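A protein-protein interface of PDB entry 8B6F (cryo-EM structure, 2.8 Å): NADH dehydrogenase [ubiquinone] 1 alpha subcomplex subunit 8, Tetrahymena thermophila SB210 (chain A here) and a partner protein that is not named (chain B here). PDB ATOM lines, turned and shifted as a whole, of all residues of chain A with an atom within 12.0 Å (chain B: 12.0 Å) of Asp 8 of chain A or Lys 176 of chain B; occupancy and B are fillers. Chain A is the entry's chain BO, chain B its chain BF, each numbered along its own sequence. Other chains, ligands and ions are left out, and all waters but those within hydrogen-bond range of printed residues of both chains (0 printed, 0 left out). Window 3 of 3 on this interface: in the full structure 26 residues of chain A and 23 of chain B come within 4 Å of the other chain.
The side-chain amino group (NZ) of Lys 173 of chain B is in salt-bridge range of the side-chain carboxylate (OD1) of Asp 12 of chain A (3.6 Å). The side-chain amino group of Lys 176 of chain B is in salt-bridge range of the side-chain carboxylate of Asp 8 of chain A, 3.2 Å away. NZ of Lys 169 of chain B is in salt-bridge range of OD1 of Asp 12 of chain A (3.99 Å). The backbone NH (N) of Asp 12 of chain A is in hydrogen-bond range of the side-chain carboxylate (OE2) of Glu 170 of chain B, at 2.7 Å. The side-chain amino group (NZ) of Lys 140 of chain B lies within hydrogen-bond range of the backbone carbonyl oxygen (O) of Asp 13 of chain A, 2.9 Å away.
Of chain B, only Lys 176 comes within 4 Å of Asp 8 of chain A. Of the printed residues of chain A, Lys 176 of chain B touches Asp 8 (3.2 Å) and Glu 10 (3.4 Å). Val 6 of chain A touches none of the printed residues of chain B. Ser 9 of chain A touches none of the printed residues of chain B. No residue of chain A comes within 4 Å of Pro 174 of chain B. No residue of chain A comes within 4 Å of Lys 177 of chain B. No residue of chain A comes within 4 Å of Ala 178 of chain B. Of the printed residues of chain B, Asp 13 of chain A touches Lys 140 (2.9 Å). Of the printed residues of chain A, Glu 170 of chain B touches Phe 11 (3.3 Å) and Asp 12 (2.7 Å). The nearest residue of chain B that does not touch Asp 8 of chain A is Lys 177 of chain B (7.4 Å). The nearest printed residue of chain A that does not touch Glu 170 of chain B is Glu 10 of chain A (4.4 Å).
OG of Ser 9 of chain A lies within hydrogen-bond range of O of Phe 11 of chain A (2.7 Å). The side-chain carboxylate (OE2) of Glu 170 of chain B is in salt-bridge range of the side-chain amino group (NZ) of Lys 173 of chain B.
Of the 11 printed residues of chain B, 5 touch a printed residue of chain A. Along chain B the printed residues that touch a printed residue of chain A span positions 140 to 176. Of the 13 printed residues of chain A, 5 touch a printed residue of chain B. Hydrophobic or aromatic side chains of chain A within 4 Å of the printed part of chain B: Phe 11. Among the printed residues, Asp or Glu carboxylates within 4 Å of a Lys or Arg side-chain nitrogen of the other chain: Asp 8 of chain A with Lys 176 of chain B (3.2 Å), Asp 12 of chain A with Lys 169 of chain B (3.99 Å) and Asp 12 of chain A with Lys 173 of chain B (3.6 Å).
Among the printed residues, pairs that only touch across the chains: Phe 11 of chain A with Glu 170 of chain B and Glu 10 of chain A with Lys 176 of chain B.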
ATOM      1  N   ASN A   4      27.573  -9.231 -28.448  1.00  0.00           N
ATOM      2  CA  ASN A   4      27.093  -9.123 -27.082  1.00  0.00           C
ATOM      3  C   ASN A   4      26.538  -7.729 -26.819  1.00  0.00           C
ATOM      4  O   ASN A   4      27.163  -6.735 -27.204  1.00  0.00           O
ATOM      5  CB  ASN A   4      28.211  -9.407 -26.074  1.00  0.00           C
ATOM      6  CG  ASN A   4      28.550 -10.878 -25.976  1.00  0.00           C
ATOM      7  OD1 ASN A   4      27.707 -11.740 -26.220  1.00  0.00           O
ATOM      8  ND2 ASN A   4      29.791 -11.174 -25.608  1.00  0.00           N
ATOM      9  N   PRO A   5      25.380  -7.614 -26.172  1.00  0.00           N
ATOM     10  CA  PRO A   5      24.850  -6.283 -25.861  1.00  0.00           C
ATOM     11  C   PRO A   5      25.706  -5.570 -24.827  1.00  0.00           C
ATOM     12  O   PRO A   5      26.369  -6.193 -23.994  1.00  0.00           O
ATOM     13  CB  PRO A   5      23.448  -6.577 -25.318  1.00  0.00           C
ATOM     14  CG  PRO A   5      23.548  -7.949 -24.765  1.00  0.00           C
ATOM     15  CD  PRO A   5      24.511  -8.683 -25.653  1.00  0.00           C
ATOM     16  N   VAL A   6      25.682  -4.243 -24.888  1.00  0.00           N
ATOM     17  CA  VAL A   6      26.408  -3.418 -23.927  1.00  0.00           C
ATOM     18  C   VAL A   6      25.532  -3.240 -22.694  1.00  0.00           C
ATOM     19  O   VAL A   6      24.418  -2.714 -22.781  1.00  0.00           O
ATOM     20  CB  VAL A   6      26.789  -2.062 -24.537  1.00  0.00           C
ATOM     21  CG1 VAL A   6      27.524  -1.201 -23.519  1.00  0.00           C
ATOM     22  CG2 VAL A   6      27.638  -2.260 -25.781  1.00  0.00           C
ATOM     23  N   LYS A   7      26.035  -3.681 -21.540  1.00  0.00           N
ATOM     24  CA  LYS A   7      25.239  -3.615 -20.319  1.00  0.00           C
ATOM     25  C   LYS A   7      24.956  -2.171 -19.926  1.00  0.00           C
ATOM     26  O   LYS A   7      23.807  -1.799 -19.665  1.00  0.00           O
ATOM     27  CB  LYS A   7      25.958  -4.355 -19.188  1.00  0.00           C
ATOM     28  CG  LYS A   7      25.170  -4.431 -17.885  1.00  0.00           C
ATOM     29  CD  LYS A   7      23.857  -5.182 -18.063  1.00  0.00           C
ATOM     30  CE  LYS A   7      23.126  -5.351 -16.741  1.00  0.00           C
ATOM     31  NZ  LYS A   7      23.891  -6.187 -15.774  1.00  0.00           N
ATOM     32  N   ASP A   8      25.996  -1.341 -19.881  1.00  0.00           N
ATOM     33  CA  ASP A   8      25.861   0.073 -19.537  1.00  0.00           C
ATOM     34  C   ASP A   8      25.958   0.868 -20.834  1.00  0.00           C
ATOM     35  O   ASP A   8      27.030   1.333 -21.221  1.00  0.00           O
ATOM     36  CB  ASP A   8      26.929   0.491 -18.532  1.00  0.00           C
ATOM     37  CG  ASP A   8      26.748   1.918 -18.048  1.00  0.00           C
ATOM     38  OD1 ASP A   8      25.726   2.542 -18.401  1.00  0.00           O
ATOM     39  OD2 ASP A   8      27.630   2.415 -17.318  1.00  0.00           O
ATOM     40  N   SER A   9      24.822   1.025 -21.506  1.00  0.00           N
ATOM     41  CA  SER A   9      24.748   1.703 -22.792  1.00  0.00           C
ATOM     42  C   SER A   9      23.932   2.977 -22.644  1.00  0.00           C
ATOM     43  O   SER A   9      22.865   2.968 -22.023  1.00  0.00           O
ATOM     44  CB  SER A   9      24.125   0.798 -23.856  1.00  0.00           C
ATOM     45  OG  SER A   9      22.800   0.438 -23.510  1.00  0.00           O
ATOM     46  N   GLU A  10      24.437   4.071 -23.217  1.00  0.00           N
ATOM     47  CA  GLU A  10      23.716   5.336 -23.154  1.00  0.00           C
ATOM     48  C   GLU A  10      22.373   5.238 -23.867  1.00  0.00           C
ATOM     49  O   GLU A  10      21.365   5.762 -23.380  1.00  0.00           O
ATOM     50  CB  GLU A  10      24.566   6.450 -23.762  1.00  0.00           C
ATOM     51  CG  GLU A  10      23.948   7.829 -23.640  1.00  0.00           C
ATOM     52  CD  GLU A  10      24.849   8.915 -24.185  1.00  0.00           C
ATOM     53  OE1 GLU A  10      25.933   8.580 -24.702  1.00  0.00           O
ATOM     54  OE2 GLU A  10      24.473  10.103 -24.096  1.00  0.00           O
ATOM     55  N   PHE A  11      22.341   4.571 -25.014  1.00  0.00           N
ATOM     56  CA  PHE A  11      21.120   4.383 -25.782  1.00  0.00           C
ATOM     57  C   PHE A  11      20.606   2.957 -25.621  1.00  0.00           C
ATOM     58  O   PHE A  11      21.297   2.067 -25.118  1.00  0.00           O
ATOM     59  CB  PHE A  11      21.362   4.718 -27.255  1.00  0.00           C
ATOM     60  CG  PHE A  11      21.636   6.171 -27.498  1.00  0.00           C
ATOM     61  CD1 PHE A  11      22.924   6.671 -27.414  1.00  0.00           C
ATOM     62  CD2 PHE A  11      20.602   7.042 -27.796  1.00  0.00           C
ATOM     63  CE1 PHE A  11      23.178   8.013 -27.630  1.00  0.00           C
ATOM     64  CE2 PHE A  11      20.849   8.384 -28.014  1.00  0.00           C
ATOM     65  CZ  PHE A  11      22.138   8.871 -27.932  1.00  0.00           C
ATOM     66  N   ASP A  12      19.366   2.746 -26.068  1.00  0.00           N
ATOM     67  CA  ASP A  12      18.643   1.529 -25.713  1.00  0.00           C
ATOM     68  C   ASP A  12      19.383   0.279 -26.173  1.00  0.00           C
ATOM     69  O   ASP A  12      19.559  -0.668 -25.400  1.00  0.00           O
ATOM     70  CB  ASP A  12      17.236   1.569 -26.307  1.00  0.00           C
ATOM     71  CG  ASP A  12      16.408   0.360 -25.920  1.00  0.00           C
ATOM     72  OD1 ASP A  12      16.099   0.211 -24.720  1.00  0.00           O
ATOM     73  OD2 ASP A  12      16.066  -0.441 -26.815  1.00  0.00           O
ATOM     74  N   ASP A  13      19.820   0.253 -27.429  1.00  0.00           N
ATOM     75  CA  ASP A  13      20.410  -0.940 -28.023  1.00  0.00           C
ATOM     76  C   ASP A  13      21.835  -0.634 -28.460  1.00  0.00           C
ATOM     77  O   ASP A  13      22.051   0.190 -29.354  1.00  0.00           O
ATOM     78  CB  ASP A  13      19.572  -1.425 -29.208  1.00  0.00           C
ATOM     79  CG  ASP A  13      19.962  -2.813 -29.668  1.00  0.00           C
ATOM     80  OD1 ASP A  13      21.142  -3.186 -29.508  1.00  0.00           O
ATOM     81  OD2 ASP A  13      19.087  -3.535 -30.190  1.00  0.00           O
ATOM     82  N   GLU A  14      22.800  -1.298 -27.829  1.00  0.00           N
ATOM     83  CA  GLU A  14      24.195  -1.244 -28.239  1.00  0.00           C
ATOM     84  C   GLU A  14      24.788  -2.636 -28.110  1.00  0.00           C
ATOM     85  O   GLU A  14      24.450  -3.376 -27.183  1.00  0.00           O
ATOM     86  CB  GLU A  14      24.999  -0.246 -27.399  1.00  0.00           C
ATOM     87  CG  GLU A  14      24.564   1.199 -27.578  1.00  0.00           C
ATOM     88  CD  GLU A  14      25.481   2.174 -26.867  1.00  0.00           C
ATOM     89  OE1 GLU A  14      26.560   1.747 -26.407  1.00  0.00           O
ATOM     90  OE2 GLU A  14      25.123   3.365 -26.764  1.00  0.00           O
ATOM     91  N   VAL A  15      25.667  -2.993 -29.043  1.00  0.00           N
ATOM     92  CA  VAL A  15      26.226  -4.337 -29.118  1.00  0.00           C
ATOM     93  C   VAL A  15      27.721  -4.243 -29.380  1.00  0.00           C
ATOM     94  O   VAL A  15      28.173  -3.417 -30.179  1.00  0.00           O
ATOM     95  CB  VAL A  15      25.531  -5.172 -30.210  1.00  0.00           C
ATOM     96  CG1 VAL A  15      24.085  -5.440 -29.836  1.00  0.00           C
ATOM     97  CG2 VAL A  15      25.608  -4.454 -31.548  1.00  0.00           C
ATOM     98  N   LYS A  16      28.485  -5.090 -28.697  1.00  0.00           N
ATOM     99  CA  LYS A  16      29.920  -5.225 -28.908  1.00  0.00           C
ATOM    100  C   LYS A  16      30.215  -6.653 -29.337  1.00  0.00           C
ATOM    101  O   LYS A  16      29.720  -7.603 -28.722  1.00  0.00           O
ATOM    102  CB  LYS A  16      30.701  -4.870 -27.641  1.00  0.00           C
ATOM    103  CG  LYS A  16      32.209  -4.989 -27.795  1.00  0.00           C
ATOM    104  CD  LYS A  16      32.932  -4.556 -26.530  1.00  0.00           C
ATOM    105  CE  LYS A  16      34.430  -4.791 -26.641  1.00  0.00           C
ATOM    106  NZ  LYS A  16      35.029  -4.076 -27.805  1.00  0.00           N
ATOM    107  N   LYS B 140      19.023   0.549 -36.206  1.00  0.00           N
ATOM    108  CA  LYS B 140      18.247   1.079 -35.090  1.00  0.00           C
ATOM    109  C   LYS B 140      17.327   2.200 -35.552  1.00  0.00           C
ATOM    110  O   LYS B 140      16.150   2.245 -35.178  1.00  0.00           O
ATOM    111  CB  LYS B 140      19.174   1.588 -33.984  1.00  0.00           C
ATOM    112  CG  LYS B 140      19.848   0.497 -33.175  1.00  0.00           C
ATOM    113  CD  LYS B 140      20.414   1.032 -31.868  1.00  0.00           C
ATOM    114  CE  LYS B 140      21.335   2.224 -32.083  1.00  0.00           C
ATOM    115  NZ  LYS B 140      21.995   2.649 -30.816  1.00  0.00           N
ATOM    116  N   LYS B 169      11.281   7.377 -27.170  1.00  0.00           N
ATOM    117  CA  LYS B 169      11.773   6.820 -25.915  1.00  0.00           C
ATOM    118  C   LYS B 169      13.162   7.352 -25.583  1.00  0.00           C
ATOM    119  O   LYS B 169      13.443   7.695 -24.429  1.00  0.00           O
ATOM    120  CB  LYS B 169      11.784   5.294 -25.990  1.00  0.00           C
ATOM    121  CG  LYS B 169      12.202   4.619 -24.695  1.00  0.00           C
ATOM    122  CD  LYS B 169      11.872   3.134 -24.702  1.00  0.00           C
ATOM    123  CE  LYS B 169      12.609   2.399 -25.814  1.00  0.00           C
ATOM    124  NZ  LYS B 169      12.327   0.937 -25.789  1.00  0.00           N
ATOM    125  N   GLU B 170      14.043   7.432 -26.582  1.00  0.00           N
ATOM    126  CA  GLU B 170      15.391   7.938 -26.341  1.00  0.00           C
ATOM    127  C   GLU B 170      15.363   9.388 -25.876  1.00  0.00           C
ATOM    128  O   GLU B 170      16.096   9.767 -24.956  1.00  0.00           O
ATOM    129  CB  GLU B 170      16.234   7.802 -27.608  1.00  0.00           C
ATOM    130  CG  GLU B 170      16.523   6.367 -28.010  1.00  0.00           C
ATOM    131  CD  GLU B 170      17.405   5.648 -27.013  1.00  0.00           C
ATOM    132  OE1 GLU B 170      17.916   6.309 -26.085  1.00  0.00           O
ATOM    133  OE2 GLU B 170      17.590   4.423 -27.156  1.00  0.00           O
ATOM    134  N   MET B 171      14.527  10.216 -26.503  1.00  0.00           N
ATOM    135  CA  MET B 171      14.408  11.608 -26.084  1.00  0.00           C
ATOM    136  C   MET B 171      13.873  11.713 -24.660  1.00  0.00           C
ATOM    137  O   MET B 171      14.366  12.516 -23.860  1.00  0.00           O
ATOM    138  CB  MET B 171      13.504  12.370 -27.053  1.00  0.00           C
ATOM    139  CG  MET B 171      14.093  12.531 -28.447  1.00  0.00           C
ATOM    140  SD  MET B 171      12.938  13.276 -29.612  1.00  0.00           S
ATOM    141  CE  MET B 171      13.917  13.270 -31.110  1.00  0.00           C
ATOM    142  N   GLN B 172      12.864  10.908 -24.323  1.00  0.00           N
ATOM    143  CA  GLN B 172      12.293  10.954 -22.982  1.00  0.00           C
ATOM    144  C   GLN B 172      13.269  10.461 -21.918  1.00  0.00           C
ATOM    145  O   GLN B 172      13.147  10.845 -20.750  1.00  0.00           O
ATOM    146  CB  GLN B 172      11.006  10.129 -22.933  1.00  0.00           C
ATOM    147  CG  GLN B 172       9.878  10.674 -23.801  1.00  0.00           C
ATOM    148  CD  GLN B 172       9.483  12.093 -23.436  1.00  0.00           C
ATOM    149  OE1 GLN B 172       9.303  12.941 -24.309  1.00  0.00           O
ATOM    150  NE2 GLN B 172       9.340  12.356 -22.140  1.00  0.00           N
ATOM    151  N   LYS B 173      14.230   9.616 -22.286  1.00  0.00           N
ATOM    152  CA  LYS B 173      15.209   9.157 -21.311  1.00  0.00           C
ATOM    153  C   LYS B 173      15.996  10.344 -20.758  1.00  0.00           C
ATOM    154  O   LYS B 173      16.223  11.332 -21.462  1.00  0.00           O
ATOM    155  CB  LYS B 173      16.167   8.147 -21.940  1.00  0.00           C
ATOM    156  CG  LYS B 173      15.602   6.740 -22.065  1.00  0.00           C
ATOM    157  CD  LYS B 173      16.621   5.788 -22.676  1.00  0.00           C
ATOM    158  CE  LYS B 173      16.032   4.400 -22.869  1.00  0.00           C
ATOM    159  NZ  LYS B 173      16.993   3.477 -23.538  1.00  0.00           N
ATOM    160  N   PRO B 174      16.417  10.281 -19.497  1.00  0.00           N
ATOM    161  CA  PRO B 174      17.159  11.395 -18.907  1.00  0.00           C
ATOM    162  C   PRO B 174      18.621  11.355 -19.313  1.00  0.00           C
ATOM    163  O   PRO B 174      19.111  10.324 -19.799  1.00  0.00           O
ATOM    164  CB  PRO B 174      16.990  11.167 -17.400  1.00  0.00           C
ATOM    165  CG  PRO B 174      16.882   9.692 -17.274  1.00  0.00           C
ATOM    166  CD  PRO B 174      16.177   9.205 -18.518  1.00  0.00           C
ATOM    167  N   PRO B 175      19.354  12.452 -19.125  1.00  0.00           N
ATOM    168  CA  PRO B 175      20.771  12.462 -19.509  1.00  0.00           C
ATOM    169  C   PRO B 175      21.581  11.466 -18.694  1.00  0.00           C
ATOM    170  O   PRO B 175      21.275  11.181 -17.534  1.00  0.00           O
ATOM    171  CB  PRO B 175      21.211  13.905 -19.223  1.00  0.00           C
ATOM    172  CG  PRO B 175      19.952  14.692 -19.138  1.00  0.00           C
ATOM    173  CD  PRO B 175      18.920  13.756 -18.600  1.00  0.00           C
ATOM    174  N   LYS B 176      22.629  10.935 -19.318  1.00  0.00           N
ATOM    175  CA  LYS B 176      23.534  10.033 -18.619  1.00  0.00           C
ATOM    176  C   LYS B 176      24.340  10.804 -17.582  1.00  0.00           C
ATOM    177  O   LYS B 176      24.894  11.868 -17.874  1.00  0.00           O
ATOM    178  CB  LYS B 176      24.469   9.343 -19.612  1.00  0.00           C
ATOM    179  CG  LYS B 176      25.577   8.531 -18.950  1.00  0.00           C
ATOM    180  CD  LYS B 176      26.385   7.730 -19.963  1.00  0.00           C
ATOM    181  CE  LYS B 176      25.619   6.524 -20.480  1.00  0.00           C
ATOM    182  NZ  LYS B 176      25.282   5.554 -19.398  1.00  0.00           N
ATOM    183  N   LYS B 177      24.406  10.262 -16.368  1.00  0.00           N
ATOM    184  CA  LYS B 177      25.160  10.892 -15.295  1.00  0.00           C
ATOM    185  C   LYS B 177      26.654  10.688 -15.501  1.00  0.00           C
ATOM    186  O   LYS B 177      27.093   9.643 -15.990  1.00  0.00           O
ATOM    187  CB  LYS B 177      24.736  10.324 -13.940  1.00  0.00           C
ATOM    188  CG  LYS B 177      23.292  10.632 -13.571  1.00  0.00           C
ATOM    189  CD  LYS B 177      22.961  10.131 -12.175  1.00  0.00           C
ATOM    190  CE  LYS B 177      21.550  10.530 -11.770  1.00  0.00           C
ATOM    191  NZ  LYS B 177      21.216  10.076 -10.389  1.00  0.00           N
ATOM    192  N   ALA B 178      27.434  11.696 -15.124  1.00  0.00           N
ATOM    193  CA  ALA B 178      28.886  11.640 -15.250  1.00  0.00           C
ATOM    194  C   ALA B 178      29.296  11.347 -16.688  1.00  0.00           C
ATOM    195  O   ALA B 178      29.461  10.189 -17.073  1.00  0.00           O
ATOM    196  CB  ALA B 178      29.461  10.589 -14.311  1.00  0.00           C
